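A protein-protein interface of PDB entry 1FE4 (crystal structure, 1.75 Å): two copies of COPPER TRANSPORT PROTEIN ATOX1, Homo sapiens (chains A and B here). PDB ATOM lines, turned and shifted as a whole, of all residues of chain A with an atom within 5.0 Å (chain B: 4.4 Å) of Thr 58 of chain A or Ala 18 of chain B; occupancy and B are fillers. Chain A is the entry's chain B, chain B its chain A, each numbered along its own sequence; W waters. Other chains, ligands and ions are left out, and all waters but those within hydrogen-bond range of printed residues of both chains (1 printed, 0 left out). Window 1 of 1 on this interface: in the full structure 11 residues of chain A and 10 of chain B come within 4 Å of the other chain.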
ATOM      1  N   ALA A  18      14.756  24.644 -20.764  1.00  0.00           N
ATOM      2  CA  ALA A  18      15.897  23.992 -21.417  1.00  0.00           C
ATOM      3  C   ALA A  18      16.006  24.385 -22.894  1.00  0.00           C
ATOM      4  O   ALA A  18      17.111  24.522 -23.424  1.00  0.00           O
ATOM      5  CB  ALA A  18      15.790  22.474 -21.281  1.00  0.00           C
ATOM      6  N   VAL A  19      14.864  24.552 -23.561  1.00  0.00           N
ATOM      7  CA  VAL A  19      14.864  24.967 -24.968  1.00  0.00           C
ATOM      8  C   VAL A  19      15.445  26.380 -25.042  1.00  0.00           C
ATOM      9  O   VAL A  19      16.239  26.700 -25.932  1.00  0.00           O
ATOM     10  CB  VAL A  19      13.419  24.956 -25.561  1.00  0.00           C
ATOM     11  CG1 VAL A  19      13.388  25.671 -26.916  1.00  0.00           C
ATOM     12  CG2 VAL A  19      12.945  23.514 -25.726  1.00  0.00           C
ATOM     13  N   VAL A  22      19.465  26.359 -24.674  1.00  0.00           N
ATOM     14  CA  VAL A  22      20.241  25.939 -25.843  1.00  0.00           C
ATOM     15  C   VAL A  22      20.193  26.988 -26.952  1.00  0.00           C
ATOM     16  O   VAL A  22      21.165  27.151 -27.694  1.00  0.00           O
ATOM     17  CB  VAL A  22      19.778  24.554 -26.416  1.00  0.00           C
ATOM     18  CG1 VAL A  22      19.896  23.476 -25.337  1.00  0.00           C
ATOM     19  CG2 VAL A  22      18.358  24.633 -26.951  1.00  0.00           C
ATOM     20  N   THR A  54      20.430  22.221 -33.341  1.00  0.00           N
ATOM     21  CA  THR A  54      20.500  22.827 -32.011  1.00  0.00           C
ATOM     22  C   THR A  54      19.319  22.381 -31.143  1.00  0.00           C
ATOM     23  O   THR A  54      19.494  22.016 -29.978  1.00  0.00           O
ATOM     24  CB  THR A  54      20.519  24.374 -32.106  1.00  0.00           C
ATOM     25  OG1 THR A  54      21.693  24.792 -32.816  1.00  0.00           O
ATOM     26  CG2 THR A  54      20.532  25.005 -30.715  1.00  0.00           C
ATOM     27  N   LEU A  55      18.119  22.399 -31.710  1.00  0.00           N
ATOM     28  CA  LEU A  55      16.936  21.985 -30.963  1.00  0.00           C
ATOM     29  C   LEU A  55      17.001  20.508 -30.568  1.00  0.00           C
ATOM     30  O   LEU A  55      16.564  20.137 -29.479  1.00  0.00           O
ATOM     31  CB  LEU A  55      15.670  22.256 -31.785  1.00  0.00           C
ATOM     32  CG  LEU A  55      15.308  23.733 -31.973  1.00  0.00           C
ATOM     33  CD1 LEU A  55      14.118  23.850 -32.927  1.00  0.00           C
ATOM     34  CD2 LEU A  55      14.972  24.366 -30.620  1.00  0.00           C
ATOM     35  N   LYS A  56      17.549  19.670 -31.444  1.00  0.00           N
ATOM     36  CA  LYS A  56      17.658  18.241 -31.160  1.00  0.00           C
ATOM     37  C   LYS A  56      18.603  17.925 -29.990  1.00  0.00           C
ATOM     38  O   LYS A  56      18.552  16.829 -29.428  1.00  0.00           O
ATOM     39  CB  LYS A  56      18.109  17.479 -32.415  1.00  0.00           C
ATOM     40  CG  LYS A  56      17.012  17.276 -33.464  1.00  0.00           C
ATOM     41  CD  LYS A  56      17.574  16.622 -34.723  1.00  0.00           C
ATOM     42  CE  LYS A  56      16.502  16.367 -35.778  1.00  0.00           C
ATOM     43  NZ  LYS A  56      15.602  15.233 -35.422  1.00  0.00           N
ATOM     44  N   LYS A  57      19.450  18.882 -29.612  1.00  0.00           N
ATOM     45  CA  LYS A  57      20.387  18.680 -28.502  1.00  0.00           C
ATOM     46  C   LYS A  57      19.672  18.517 -27.160  1.00  0.00           C
ATOM     47  O   LYS A  57      20.245  17.995 -26.200  1.00  0.00           O
ATOM     48  CB  LYS A  57      21.374  19.850 -28.411  1.00  0.00           C
ATOM     49  CG  LYS A  57      22.371  19.911 -29.553  1.00  0.00           C
ATOM     50  CD  LYS A  57      23.290  21.115 -29.427  1.00  0.00           C
ATOM     51  CE  LYS A  57      24.321  21.125 -30.547  1.00  0.00           C
ATOM     52  NZ  LYS A  57      25.211  22.314 -30.472  1.00  0.00           N
ATOM     53  N   THR A  58      18.424  18.966 -27.100  1.00  0.00           N
ATOM     54  CA  THR A  58      17.627  18.873 -25.882  1.00  0.00           C
ATOM     55  C   THR A  58      17.229  17.430 -25.570  1.00  0.00           C
ATOM     56  O   THR A  58      16.919  17.101 -24.424  1.00  0.00           O
ATOM     57  CB  THR A  58      16.317  19.669 -26.008  1.00  0.00           C
ATOM     58  OG1 THR A  58      15.561  19.146 -27.109  1.00  0.00           O
ATOM     59  CG2 THR A  58      16.593  21.154 -26.234  1.00  0.00           C
ATOM     60  N   GLY A  59      17.230  16.582 -26.596  1.00  0.00           N
ATOM     61  CA  GLY A  59      16.825  15.197 -26.420  1.00  0.00           C
ATOM     62  C   GLY A  59      15.336  15.031 -26.705  1.00  0.00           C
ATOM     63  O   GLY A  59      14.784  13.932 -26.594  1.00  0.00           O
ATOM     64  N   LYS A  60      14.684  16.131 -27.073  1.00  0.00           N
ATOM     65  CA  LYS A  60      13.253  16.128 -27.382  1.00  0.00           C
ATOM     66  C   LYS A  60      13.023  15.779 -28.859  1.00  0.00           C
ATOM     67  O   LYS A  60      13.939  15.888 -29.678  1.00  0.00           O
ATOM     68  CB  LYS A  60      12.650  17.509 -27.096  1.00  0.00           C
ATOM     69  CG  LYS A  60      12.970  18.084 -25.715  1.00  0.00           C
ATOM     70  CD  LYS A  60      12.348  17.267 -24.593  1.00  0.00           C
ATOM     71  CE  LYS A  60      10.832  17.398 -24.575  1.00  0.00           C
ATOM     72  NZ  LYS A  60      10.204  16.566 -23.503  1.00  0.00           N
ATOM     73  N   GLY B  14       8.954  13.556 -19.128  1.00  0.00           N
ATOM     74  CA  GLY B  14       9.563  13.954 -20.385  1.00  0.00           C
ATOM     75  C   GLY B  14      11.013  14.374 -20.215  1.00  0.00           C
ATOM     76  O   GLY B  14      11.829  14.173 -21.116  1.00  0.00           O
ATOM     77  N   CYS B  15      11.335  14.970 -19.068  1.00  0.00           N
ATOM     78  CA  CYS B  15      12.706  15.396 -18.786  1.00  0.00           C
ATOM     79  C   CYS B  15      13.619  14.177 -18.666  1.00  0.00           C
ATOM     80  O   CYS B  15      14.757  14.186 -19.152  1.00  0.00           O
ATOM     81  CB  CYS B  15      12.770  16.211 -17.482  1.00  0.00           C
ATOM     82  SG  CYS B  15      12.170  17.933 -17.578  1.00  0.00           S
ATOM     83  N   ALA B  16      13.120  13.130 -18.016  1.00  0.00           N
ATOM     84  CA  ALA B  16      13.889  11.899 -17.831  1.00  0.00           C
ATOM     85  C   ALA B  16      14.105  11.185 -19.161  1.00  0.00           C
ATOM     86  O   ALA B  16      15.186  10.657 -19.428  1.00  0.00           O
ATOM     87  CB  ALA B  16      13.169  10.969 -16.850  1.00  0.00           C
ATOM     88  N   GLU B  17      13.073  11.162 -19.998  1.00  0.00           N
ATOM     89  CA  GLU B  17      13.190  10.507 -21.295  1.00  0.00           C
ATOM     90  C   GLU B  17      14.228  11.208 -22.174  1.00  0.00           C
ATOM     91  O   GLU B  17      14.967  10.549 -22.909  1.00  0.00           O
ATOM     92  CB  GLU B  17      11.837  10.482 -22.008  1.00  0.00           C
ATOM     93  CG  GLU B  17      11.857   9.723 -23.326  1.00  0.00           C
ATOM     94  CD  GLU B  17      10.473   9.524 -23.912  1.00  0.00           C
ATOM     95  OE1 GLU B  17       9.776  10.529 -24.156  1.00  0.00           O
ATOM     96  OE2 GLU B  17      10.086   8.355 -24.128  1.00  0.00           O
ATOM     97  N   ALA B  18      14.283  12.537 -22.094  1.00  0.00           N
ATOM     98  CA  ALA B  18      15.234  13.316 -22.889  1.00  0.00           C
ATOM     99  C   ALA B  18      16.668  12.990 -22.493  1.00  0.00           C
ATOM    100  O   ALA B  18      17.553  12.891 -23.347  1.00  0.00           O
ATOM    101  CB  ALA B  18      14.969  14.817 -22.717  1.00  0.00           C
ATOM    102  N   VAL B  19      16.902  12.830 -21.194  1.00  0.00           N
ATOM    103  CA  VAL B  19      18.235  12.488 -20.709  1.00  0.00           C
ATOM    104  C   VAL B  19      18.650  11.123 -21.269  1.00  0.00           C
ATOM    105  O   VAL B  19      19.786  10.946 -21.719  1.00  0.00           O
ATOM    106  CB  VAL B  19      18.274  12.449 -19.154  1.00  0.00           C
ATOM    107  CG1 VAL B  19      19.611  11.889 -18.669  1.00  0.00           C
ATOM    108  CG2 VAL B  19      18.070  13.853 -18.596  1.00  0.00           C
ATOM    109  N   SER B  20      17.727  10.163 -21.259  1.00  0.00           N
ATOM    110  CA  SER B  20      18.028   8.823 -21.760  1.00  0.00           C
ATOM    111  C   SER B  20      18.379   8.816 -23.245  1.00  0.00           C
ATOM    112  O   SER B  20      19.202   8.015 -23.689  1.00  0.00           O
ATOM    113  CB  SER B  20      16.857   7.864 -21.503  1.00  0.00           C
ATOM    114  OG  SER B  20      15.776   8.077 -22.400  1.00  0.00           O
ATOM    115  N   ARG B  21      17.764   9.710 -24.014  1.00  0.00           N
ATOM    116  CA  ARG B  21      18.034   9.772 -25.449  1.00  0.00           C
ATOM    117  C   ARG B  21      19.430  10.288 -25.793  1.00  0.00           C
ATOM    118  O   ARG B  21      20.103   9.725 -26.662  1.00  0.00           O
ATOM    119  CB  ARG B  21      16.981  10.631 -26.151  1.00  0.00           C
ATOM    120  CG  ARG B  21      15.610   9.990 -26.193  1.00  0.00           C
ATOM    121  CD  ARG B  21      14.615  10.878 -26.909  1.00  0.00           C
ATOM    122  NE  ARG B  21      13.301  10.254 -27.002  1.00  0.00           N
ATOM    123  CZ  ARG B  21      12.226  10.856 -27.499  1.00  0.00           C
ATOM    124  NH1 ARG B  21      12.314  12.101 -27.947  1.00  0.00           N
ATOM    125  NH2 ARG B  21      11.064  10.216 -27.546  1.00  0.00           N
ATOM    126  N   VAL B  22      19.876  11.349 -25.126  1.00  0.00           N
ATOM    127  CA  VAL B  22      21.200  11.876 -25.423  1.00  0.00           C
ATOM    128  C   VAL B  22      22.285  10.888 -24.999  1.00  0.00           C
ATOM    129  O   VAL B  22      23.345  10.823 -25.629  1.00  0.00           O
ATOM    130  CB  VAL B  22      21.438  13.266 -24.766  1.00  0.00           C
ATOM    131  CG1 VAL B  22      20.401  14.264 -25.288  1.00  0.00           C
ATOM    132  CG2 VAL B  22      21.377  13.169 -23.251  1.00  0.00           C
ATOM    133  N   THR B  58      21.975  19.431 -23.070  1.00  0.00           N
ATOM    134  CA  THR B  58      20.517  19.298 -23.063  1.00  0.00           C
ATOM    135  C   THR B  58      19.832  20.589 -22.613  1.00  0.00           C
ATOM    136  O   THR B  58      18.627  20.758 -22.800  1.00  0.00           O
ATOM    137  CB  THR B  58      20.042  18.177 -22.113  1.00  0.00           C
ATOM    138  OG1 THR B  58      20.356  18.531 -20.757  1.00  0.00           O
ATOM    139  CG2 THR B  58      20.705  16.857 -22.468  1.00  0.00           C
HETATM  140  O   HOH W   1      16.328  19.315 -22.466  1.00  0.00           O
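The guanidinium group of Arg 21 of chain B lies close to the backbone carbonyl oxygen of Gly 59 of chain A, 3.4 Å away.
OG1 of Thr 58 of chain A is in hydrogen-bond range of O of Leu 55 of chain A (2.8 Å).
The side-chain hydroxyl (OG1) of Thr 58 of chain A lies close to the backbone NH (N) of Lys 60 of chain A (3.1 Å).
The side-chain carboxylate (OE1) of Glu 17 of chain B is in salt-bridge range of the guanidinium group (NH2) of Arg 21 of chain B (3.6 Å).
Among the printed residues, merely in contact across the chains: Ala 18 of chain A with Thr 58 of chain B (3.6 Å), Val 22 of chain A with Thr 58 of chain B (3.9 Å), Lys 57 of chain A with Val 22 of chain B (3.8 Å), Lys 57 of chain A with Thr 58 of chain B (3.4 Å), Thr 58 of chain A with Ala 18 of chain B (3.5 Å), Thr 58 of chain A with Thr 58 of chain B (3.7 Å), Gly 59 of chain A with Ala 18 of chain B (3.8 Å), Gly 59 of chain A with Val 22 of chain B (3.9 Å), Lys 60 of chain A with Gly 14 of chain B (3.8 Å) and Lys 60 of chain A with Arg 21 of chain B (3.9 Å).
Thr 58 of chain A touches two residues of chain B.
Ala 18 of chain B touches just these residues of chain A: Thr 58 (3.5 Å) and Gly 59 (3.8 Å).
Printed residues of chain B within 4 Å of Val 22 of chain A: Thr 58.
Printed residues of chain A within 4 Å of Val 22 of chain B: Lys 57 and Gly 59.
Printed residues of chain B within 4 Å of Gly 59 of chain A: Ala 18 (3.8 Å), Arg 21 (3.1 Å) and Val 22 (3.9 Å).
Glu 17 of chain B touches none of the printed residues of chain A.
The nearest printed residue of chain B that does not touch Thr 58 of chain A is Val 22 of chain B (4.5 Å).
The nearest printed residue of chain A that does not touch Arg 21 of chain B is Thr 58 of chain A (6.7 Å).
Of the 10 printed residues of chain A, 6 touch a printed residue of chain B.
Hydrophobic or aromatic side chains of chain A that line the printed part of chain B: Ala 18 and Val 22.
Along chain A the printed residues that touch a printed residue of chain B span positions 18 to 60.
Among the printed residues, 11 pairs touch across the chains.
Ala 18 of chain A touches Thr 58 of chain B, and with the chains exchanged Thr 58 of chain A touches Ala 18 of chain B.
Val 22 of chain A touches Thr 58 of chain B, but with the chains exchanged Thr 58 of chain A does not touch Val 22 of chain B (4.5 Å).
Thr 58 of chain B touches its own counterpart, Thr 58 of chain A.
Positions printed for both chains: 18, 19, 22 and 58.
Of the 11 pairs that touch across the chains among the printed residues, 3 have their exchanged pair printed and touching as well.
Water W1 bridges O of Thr 58 of chain B (2.7 Å) and O of Thr 58 of chain A (3.0 Å).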
